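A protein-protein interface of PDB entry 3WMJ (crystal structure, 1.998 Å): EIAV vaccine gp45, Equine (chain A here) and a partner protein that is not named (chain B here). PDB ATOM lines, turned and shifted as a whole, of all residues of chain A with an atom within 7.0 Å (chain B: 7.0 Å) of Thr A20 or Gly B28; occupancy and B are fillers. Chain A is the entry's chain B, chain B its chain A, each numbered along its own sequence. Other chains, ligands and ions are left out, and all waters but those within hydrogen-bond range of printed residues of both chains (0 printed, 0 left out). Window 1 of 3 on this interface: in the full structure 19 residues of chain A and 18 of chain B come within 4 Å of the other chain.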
ATOM      1  N   HIS A  15      26.490  28.734  10.123  1.00  0.00           N
ATOM      2  CA  HIS A  15      26.383  30.017   9.436  1.00  0.00           C
ATOM      3  C   HIS A  15      26.761  29.929   7.951  1.00  0.00           C
ATOM      4  O   HIS A  15      26.085  30.517   7.099  1.00  0.00           O
ATOM      5  CB  HIS A  15      27.223  31.088  10.119  1.00  0.00           C
ATOM      6  CG  HIS A  15      27.096  32.436   9.479  1.00  0.00           C
ATOM      7  ND1 HIS A  15      25.909  33.139   9.461  1.00  0.00           N
ATOM      8  CD2 HIS A  15      27.993  33.194   8.804  1.00  0.00           C
ATOM      9  CE1 HIS A  15      26.087  34.281   8.816  1.00  0.00           C
ATOM     10  NE2 HIS A  15      27.343  34.338   8.409  1.00  0.00           N
ATOM     11  N   ASP A  16      27.831  29.206   7.629  1.00  0.00           N
ATOM     12  CA  ASP A  16      28.249  29.099   6.233  1.00  0.00           C
ATOM     13  C   ASP A  16      27.212  28.385   5.363  1.00  0.00           C
ATOM     14  O   ASP A  16      27.033  28.729   4.195  1.00  0.00           O
ATOM     15  CB  ASP A  16      29.596  28.392   6.119  1.00  0.00           C
ATOM     16  CG  ASP A  16      30.742  29.186   6.750  1.00  0.00           C
ATOM     17  OD1 ASP A  16      30.617  30.428   6.909  1.00  0.00           O
ATOM     18  OD2 ASP A  16      31.773  28.553   7.077  1.00  0.00           O
ATOM     19  N   ILE A  17      26.541  27.381   5.922  1.00  0.00           N
ATOM     20  CA  ILE A  17      25.540  26.641   5.158  1.00  0.00           C
ATOM     21  C   ILE A  17      24.315  27.510   4.889  1.00  0.00           C
ATOM     22  O   ILE A  17      23.750  27.480   3.792  1.00  0.00           O
ATOM     23  CB  ILE A  17      25.140  25.346   5.872  1.00  0.00           C
ATOM     24  CG1 ILE A  17      26.296  24.377   5.763  1.00  0.00           C
ATOM     25  CG2 ILE A  17      23.898  24.727   5.233  1.00  0.00           C
ATOM     26  CD1 ILE A  17      26.203  23.224   6.679  1.00  0.00           C
ATOM     27  N   LEU A  18      23.921  28.297   5.889  1.00  0.00           N
ATOM     28  CA  LEU A  18      22.810  29.236   5.750  1.00  0.00           C
ATOM     29  C   LEU A  18      23.075  30.194   4.603  1.00  0.00           C
ATOM     30  O   LEU A  18      22.230  30.371   3.722  1.00  0.00           O
ATOM     31  CB  LEU A  18      22.616  30.034   7.045  1.00  0.00           C
ATOM     32  CG  LEU A  18      21.622  29.427   8.022  1.00  0.00           C
ATOM     33  CD1 LEU A  18      21.587  30.218   9.326  1.00  0.00           C
ATOM     34  CD2 LEU A  18      20.252  29.403   7.360  1.00  0.00           C
ATOM     35  N   THR A  19      24.256  30.805   4.609  1.00  0.00           N
ATOM     36  CA  THR A  19      24.630  31.732   3.545  1.00  0.00           C
ATOM     37  C   THR A  19      24.694  31.014   2.187  1.00  0.00           C
ATOM     38  O   THR A  19      24.208  31.532   1.183  1.00  0.00           O
ATOM     39  CB  THR A  19      25.957  32.467   3.856  1.00  0.00           C
ATOM     40  OG1 THR A  19      27.024  31.523   3.980  1.00  0.00           O
ATOM     41  CG2 THR A  19      25.850  33.230   5.160  1.00  0.00           C
ATOM     42  N   THR A  20      25.268  29.812   2.176  1.00  0.00           N
ATOM     43  CA  THR A  20      25.422  29.023   0.949  1.00  0.00           C
ATOM     44  C   THR A  20      24.077  28.627   0.335  1.00  0.00           C
ATOM     45  O   THR A  20      23.907  28.725  -0.883  1.00  0.00           O
ATOM     46  CB  THR A  20      26.277  27.758   1.183  1.00  0.00           C
ATOM     47  OG1 THR A  20      27.592  28.138   1.593  1.00  0.00           O
ATOM     48  CG2 THR A  20      26.402  26.945  -0.088  1.00  0.00           C
ATOM     49  N   LEU A  21      23.131  28.175   1.157  1.00  0.00           N
ATOM     50  CA  LEU A  21      21.798  27.854   0.646  1.00  0.00           C
ATOM     51  C   LEU A  21      21.113  29.113   0.133  1.00  0.00           C
ATOM     52  O   LEU A  21      20.462  29.075  -0.903  1.00  0.00           O
ATOM     53  CB  LEU A  21      20.927  27.187   1.711  1.00  0.00           C
ATOM     54  CG  LEU A  21      21.356  25.795   2.189  1.00  0.00           C
ATOM     55  CD1 LEU A  21      20.550  25.379   3.418  1.00  0.00           C
ATOM     56  CD2 LEU A  21      21.170  24.790   1.072  1.00  0.00           C
ATOM     57  N   HIS A  22      21.255  30.229   0.848  1.00  0.00           N
ATOM     58  CA  HIS A  22      20.637  31.483   0.396  1.00  0.00           C
ATOM     59  C   HIS A  22      21.184  31.921  -0.972  1.00  0.00           C
ATOM     60  O   HIS A  22      20.446  32.404  -1.841  1.00  0.00           O
ATOM     61  CB  HIS A  22      20.834  32.590   1.436  1.00  0.00           C
ATOM     62  CG  HIS A  22      20.173  33.881   1.073  1.00  0.00           C
ATOM     63  ND1 HIS A  22      20.842  34.902   0.425  1.00  0.00           N
ATOM     64  CD2 HIS A  22      18.906  34.319   1.254  1.00  0.00           C
ATOM     65  CE1 HIS A  22      20.011  35.912   0.226  1.00  0.00           C
ATOM     66  NE2 HIS A  22      18.830  35.581   0.721  1.00  0.00           N
ATOM     67  N   THR A  23      22.485  31.745  -1.159  1.00  0.00           N
ATOM     68  CA  THR A  23      23.131  32.078  -2.425  1.00  0.00           C
ATOM     69  C   THR A  23      22.705  31.144  -3.556  1.00  0.00           C
ATOM     70  O   THR A  23      22.473  31.587  -4.684  1.00  0.00           O
ATOM     71  CB  THR A  23      24.643  32.002  -2.254  1.00  0.00           C
ATOM     72  OG1 THR A  23      25.023  32.918  -1.224  1.00  0.00           O
ATOM     73  CG2 THR A  23      25.363  32.348  -3.545  1.00  0.00           C
ATOM     74  N   ALA A  24      22.628  29.849  -3.252  1.00  0.00           N
ATOM     75  CA  ALA A  24      22.167  28.861  -4.217  1.00  0.00           C
ATOM     76  C   ALA A  24      20.768  29.226  -4.684  1.00  0.00           C
ATOM     77  O   ALA A  24      20.504  29.247  -5.881  1.00  0.00           O
ATOM     78  CB  ALA A  24      22.170  27.481  -3.591  1.00  0.00           C
ATOM     79  N   ARG A  25      19.872  29.516  -3.742  1.00  0.00           N
ATOM     80  CA  ARG A  25      18.485  29.809  -4.111  1.00  0.00           C
ATOM     81  C   ARG A  25      18.401  31.114  -4.884  1.00  0.00           C
ATOM     82  O   ARG A  25      17.644  31.220  -5.843  1.00  0.00           O
ATOM     83  CB  ARG A  25      17.563  29.858  -2.883  1.00  0.00           C
ATOM     84  CG  ARG A  25      17.224  28.487  -2.317  1.00  0.00           C
ATOM     85  CD  ARG A  25      16.174  28.548  -1.223  1.00  0.00           C
ATOM     86  NE  ARG A  25      15.689  27.213  -0.864  1.00  0.00           N
ATOM     87  CZ  ARG A  25      15.909  26.637   0.315  1.00  0.00           C
ATOM     88  NH1 ARG A  25      16.612  27.285   1.241  1.00  0.00           N
ATOM     89  NH2 ARG A  25      15.440  25.418   0.569  1.00  0.00           N
ATOM     90  N   ASN A  26      19.174  32.109  -4.470  1.00  0.00           N
ATOM     91  CA  ASN A  26      19.187  33.373  -5.191  1.00  0.00           C
ATOM     92  C   ASN A  26      19.689  33.204  -6.633  1.00  0.00           C
ATOM     93  O   ASN A  26      19.129  33.780  -7.576  1.00  0.00           O
ATOM     94  CB  ASN A  26      20.038  34.399  -4.450  1.00  0.00           C
ATOM     95  CG  ASN A  26      19.911  35.779  -5.045  1.00  0.00           C
ATOM     96  OD1 ASN A  26      20.874  36.334  -5.580  1.00  0.00           O
ATOM     97  ND2 ASN A  26      18.703  36.328  -4.991  1.00  0.00           N
ATOM     98  N   ASN A  27      20.741  32.412  -6.813  1.00  0.00           N
ATOM     99  CA  ASN A  27      21.218  32.127  -8.163  1.00  0.00           C
ATOM    100  C   ASN A  27      20.167  31.364  -8.973  1.00  0.00           C
ATOM    101  O   ASN A  27      19.954  31.656 -10.147  1.00  0.00           O
ATOM    102  CB  ASN A  27      22.560  31.386  -8.119  1.00  0.00           C
ATOM    103  CG  ASN A  27      23.725  32.323  -7.868  1.00  0.00           C
ATOM    104  OD1 ASN A  27      23.796  33.396  -8.458  1.00  0.00           O
ATOM    105  ND2 ASN A  27      24.630  31.933  -6.981  1.00  0.00           N
ATOM    106  N   GLU B  22      25.153  25.033  -9.180  1.00  0.00           N
ATOM    107  CA  GLU B  22      25.849  23.760  -9.021  1.00  0.00           C
ATOM    108  C   GLU B  22      27.043  23.895  -8.091  1.00  0.00           C
ATOM    109  O   GLU B  22      27.240  23.064  -7.210  1.00  0.00           O
ATOM    110  CB  GLU B  22      26.282  23.228 -10.394  1.00  0.00           C
ATOM    111  CG  GLU B  22      25.062  22.820 -11.226  1.00  0.00           C
ATOM    112  CD  GLU B  22      25.376  22.363 -12.632  1.00  0.00           C
ATOM    113  OE1 GLU B  22      26.465  22.691 -13.165  1.00  0.00           O
ATOM    114  OE2 GLU B  22      24.500  21.680 -13.219  1.00  0.00           O
ATOM    115  N   ASN B  23      27.837  24.945  -8.290  1.00  0.00           N
ATOM    116  CA  ASN B  23      28.958  25.245  -7.399  1.00  0.00           C
ATOM    117  C   ASN B  23      28.472  25.473  -5.952  1.00  0.00           C
ATOM    118  O   ASN B  23      29.049  24.916  -4.996  1.00  0.00           O
ATOM    119  CB  ASN B  23      29.736  26.472  -7.908  1.00  0.00           C
ATOM    120  CG  ASN B  23      30.921  26.831  -7.017  1.00  0.00           C
ATOM    121  OD1 ASN B  23      31.828  26.019  -6.827  1.00  0.00           O
ATOM    122  ND2 ASN B  23      30.924  28.052  -6.482  1.00  0.00           N
ATOM    123  N   ASN B  24      27.412  26.265  -5.782  1.00  0.00           N
ATOM    124  CA  ASN B  24      26.867  26.499  -4.438  1.00  0.00           C
ATOM    125  C   ASN B  24      26.412  25.193  -3.786  1.00  0.00           C
ATOM    126  O   ASN B  24      26.554  24.998  -2.572  1.00  0.00           O
ATOM    127  CB  ASN B  24      25.652  27.445  -4.454  1.00  0.00           C
ATOM    128  CG  ASN B  24      25.962  28.838  -4.996  1.00  0.00           C
ATOM    129  OD1 ASN B  24      25.107  29.450  -5.642  1.00  0.00           O
ATOM    130  ND2 ASN B  24      27.157  29.359  -4.708  1.00  0.00           N
ATOM    131  N   THR B  25      25.830  24.304  -4.583  1.00  0.00           N
ATOM    132  CA  THR B  25      25.219  23.097  -4.023  1.00  0.00           C
ATOM    133  C   THR B  25      26.291  22.087  -3.633  1.00  0.00           C
ATOM    134  O   THR B  25      26.180  21.409  -2.617  1.00  0.00           O
ATOM    135  CB  THR B  25      24.240  22.457  -5.006  1.00  0.00           C
ATOM    136  OG1 THR B  25      23.222  23.410  -5.326  1.00  0.00           O
ATOM    137  CG2 THR B  25      23.571  21.274  -4.343  1.00  0.00           C
ATOM    138  N   ILE B  26      27.336  21.999  -4.449  1.00  0.00           N
ATOM    139  CA  ILE B  26      28.471  21.131  -4.139  1.00  0.00           C
ATOM    140  C   ILE B  26      29.184  21.642  -2.883  1.00  0.00           C
ATOM    141  O   ILE B  26      29.598  20.852  -2.019  1.00  0.00           O
ATOM    142  CB  ILE B  26      29.463  21.052  -5.333  1.00  0.00           C
ATOM    143  CG1 ILE B  26      28.790  20.408  -6.547  1.00  0.00           C
ATOM    144  CG2 ILE B  26      30.684  20.230  -4.955  1.00  0.00           C
ATOM    145  CD1 ILE B  26      29.447  20.754  -7.894  1.00  0.00           C
ATOM    146  N   ASN B  27      29.327  22.960  -2.776  1.00  0.00           N
ATOM    147  CA  ASN B  27      29.926  23.560  -1.593  1.00  0.00           C
ATOM    148  C   ASN B  27      29.068  23.321  -0.343  1.00  0.00           C
ATOM    149  O   ASN B  27      29.590  23.082   0.752  1.00  0.00           O
ATOM    150  CB  ASN B  27      30.165  25.058  -1.810  1.00  0.00           C
ATOM    151  CG  ASN B  27      31.286  25.336  -2.795  1.00  0.00           C
ATOM    152  OD1 ASN B  27      32.081  24.447  -3.131  1.00  0.00           O
ATOM    153  ND2 ASN B  27      31.352  26.580  -3.278  1.00  0.00           N
ATOM    154  N   GLY B  28      27.753  23.390  -0.509  1.00  0.00           N
ATOM    155  CA  GLY B  28      26.846  23.121   0.592  1.00  0.00           C
ATOM    156  C   GLY B  28      26.964  21.690   1.082  1.00  0.00           C
ATOM    157  O   GLY B  28      26.932  21.444   2.292  1.00  0.00           O
ATOM    158  N   LEU B  29      27.074  20.750   0.144  1.00  0.00           N
ATOM    159  CA  LEU B  29      27.234  19.347   0.469  1.00  0.00           C
ATOM    160  C   LEU B  29      28.528  19.190   1.221  1.00  0.00           C
ATOM    161  O   LEU B  29      28.592  18.470   2.207  1.00  0.00           O
ATOM    162  CB  LEU B  29      27.317  18.507  -0.802  1.00  0.00           C
ATOM    163  CG  LEU B  29      26.090  17.713  -1.206  1.00  0.00           C
ATOM    164  CD1 LEU B  29      26.340  17.065  -2.571  1.00  0.00           C
ATOM    165  CD2 LEU B  29      25.767  16.658  -0.144  1.00  0.00           C
ATOM    166  N   GLU B  30      29.569  19.867   0.747  1.00  0.00           N
ATOM    167  CA  GLU B  30      30.878  19.764   1.383  1.00  0.00           C
ATOM    168  C   GLU B  30      30.826  20.291   2.813  1.00  0.00           C
ATOM    169  O   GLU B  30      31.492  19.756   3.701  1.00  0.00           O
ATOM    170  CB  GLU B  30      31.929  20.515   0.564  1.00  0.00           C
ATOM    171  CG  GLU B  30      33.343  20.385   1.115  1.00  0.00           C
ATOM    172  CD  GLU B  30      34.400  20.795   0.101  1.00  0.00           C
ATOM    173  OE1 GLU B  30      34.453  21.998  -0.261  1.00  0.00           O
ATOM    174  OE2 GLU B  30      35.171  19.908  -0.334  1.00  0.00           O
ATOM    175  N   LEU B  31      30.016  21.320   3.042  1.00  0.00           N
ATOM    176  CA  LEU B  31      29.882  21.879   4.390  1.00  0.00           C
ATOM    177  C   LEU B  31      29.126  20.946   5.332  1.00  0.00           C
ATOM    178  O   LEU B  31      29.513  20.801   6.496  1.00  0.00           O
ATOM    179  CB  LEU B  31      29.219  23.253   4.365  1.00  0.00           C
ATOM    180  CG  LEU B  31      30.015  24.387   3.723  1.00  0.00           C
ATOM    181  CD1 LEU B  31      29.099  25.590   3.564  1.00  0.00           C
ATOM    182  CD2 LEU B  31      31.189  24.739   4.600  1.00  0.00           C
ATOM    183  N   THR B  32      28.040  20.336   4.850  1.00  0.00           N
ATOM    184  CA  THR B  32      27.286  19.388   5.672  1.00  0.00           C
ATOM    185  C   THR B  32      28.174  18.211   6.008  1.00  0.00           C
ATOM    186  O   THR B  32      28.105  17.675   7.107  1.00  0.00           O
ATOM    187  CB  THR B  32      26.010  18.865   5.006  1.00  0.00           C
ATOM    188  OG1 THR B  32      26.339  18.243   3.750  1.00  0.00           O
ATOM    189  CG2 THR B  32      25.019  20.012   4.777  1.00  0.00           C
ATOM    190  N   GLU B  33      29.022  17.817   5.063  1.00  0.00           N
ATOM    191  CA  GLU B  33      29.937  16.710   5.317  1.00  0.00           C
ATOM    192  C   GLU B  33      30.934  17.043   6.411  1.00  0.00           C
ATOM    193  O   GLU B  33      31.298  16.177   7.227  1.00  0.00           O
ATOM    194  CB  GLU B  33      30.663  16.278   4.040  1.00  0.00           C
ATOM    195  CG  GLU B  33      31.634  15.104   4.254  1.00  0.00           C
ATOM    196  CD  GLU B  33      30.924  13.803   4.625  1.00  0.00           C
ATOM    197  OE1 GLU B  33      29.671  13.769   4.625  1.00  0.00           O
ATOM    198  OE2 GLU B  33      31.612  12.800   4.924  1.00  0.00           O
ATOM    199  N   GLU B  34      31.365  18.298   6.455  1.00  0.00           N
ATOM    200  CA  GLU B  34      32.263  18.727   7.519  1.00  0.00           C
ATOM    201  C   GLU B  34      31.566  18.699   8.877  1.00  0.00           C
ATOM    202  O   GLU B  34      32.168  18.312   9.873  1.00  0.00           O
ATOM    203  CB  GLU B  34      32.819  20.123   7.238  1.00  0.00           C
ATOM    204  CG  GLU B  34      33.760  20.171   6.050  1.00  0.00           C
ATOM    205  CD  GLU B  34      34.577  21.450   6.032  1.00  0.00           C
ATOM    206  OE1 GLU B  34      34.693  22.096   7.106  1.00  0.00           O
ATOM    207  OE2 GLU B  34      35.102  21.807   4.950  1.00  0.00           O
ATOM    208  N   GLN B  35      30.299  19.099   8.921  1.00  0.00           N
ATOM    209  CA  GLN B  35      29.538  19.019  10.171  1.00  0.00           C
ATOM    210  C   GLN B  35      29.371  17.571  10.611  1.00  0.00           C
ATOM    211  O   GLN B  35      29.402  17.264  11.803  1.00  0.00           O
ATOM    212  CB  GLN B  35      28.154  19.614   9.980  1.00  0.00           C
ATOM    213  CG  GLN B  35      28.125  21.123   9.880  1.00  0.00           C
ATOM    214  CD  GLN B  35      26.752  21.565   9.520  1.00  0.00           C
ATOM    215  OE1 GLN B  35      26.165  21.022   8.582  1.00  0.00           O
ATOM    216  NE2 GLN B  35      26.192  22.490  10.286  1.00  0.00           N
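The side-chain amide oxygen (OD1) of Asn B24 lies close to the backbone NH (N) of Ala A24, 3.5 Å away.
ND2 of Asn A27 is in hydrogen-bond range of OD1 of Asn B24 (2.9 Å).
The backbone carbonyl oxygen of Asp A16 lies within hydrogen-bond range of the side-chain hydroxyl of Thr A19, at 2.8 Å.
The side-chain amide nitrogen (ND2) of Asn A27 is in hydrogen-bond range of the backbone carbonyl oxygen (O) of Thr A23, at 3.2 Å.
OG1 of Thr B32 lies within hydrogen-bond range of O of Leu B29 (2.7 Å).
O of Asp A16 sits at hydrogen-bond distance from OG1 of Thr A20, at 2.7 Å.
The backbone carbonyl oxygen (O) of Thr A19 is in hydrogen-bond range of the side-chain hydroxyl (OG1) of Thr A23 (2.9 Å).
Asp A16 touches Leu B31.
CB of Leu B31 touches CG1 of Ile A17 (3.4 Å).
Ile A17 touches Thr B32 (CD1 to N, 3.9 Å).
Ile A17 touches Gln B35.
Asn B24 touches Thr A20 (O to CG2, 3.2 Å).
N of Gly B28 touches CG2 of Thr A20, at 3.8 Å.
Thr A20 touches Leu B31.
OD1 of Asn B24 touches O of Thr A23, 3.5 Å away.
Of chain A, only Thr A20 (3.8 Å) comes within 4 Å of Gly B28.
Of the printed residues of chain A, Leu B31 touches Asp A16, Ile A17 and Thr A20.
Printed residues of chain B within 4 Å of Thr A23: Asn B24 (3.5 Å).
Glu B30 touches none of the printed residues of chain A.
The nearest residue of chain A that does not touch Gly B28 is Ile A17 (4.6 Å).
Of the 14 printed residues of chain B, 5 touch a printed residue of chain A.
Printed residues of chain B that touch a printed residue of chain A: Asn B24, Gly B28, Leu B31, Thr B32 and Gln B35.
Of the 13 printed residues of chain A, 6 touch a printed residue of chain B.
Hydrophobic or aromatic side chains of chain A that line the printed part of chain B: Ile A17 and Ala A24.
Among the printed residues, 10 pairs touch across the chains.
Among the printed residues, no Asp or Glu carboxylate lies within 4 Å of a Lys or Arg side-chain nitrogen of the other chain.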
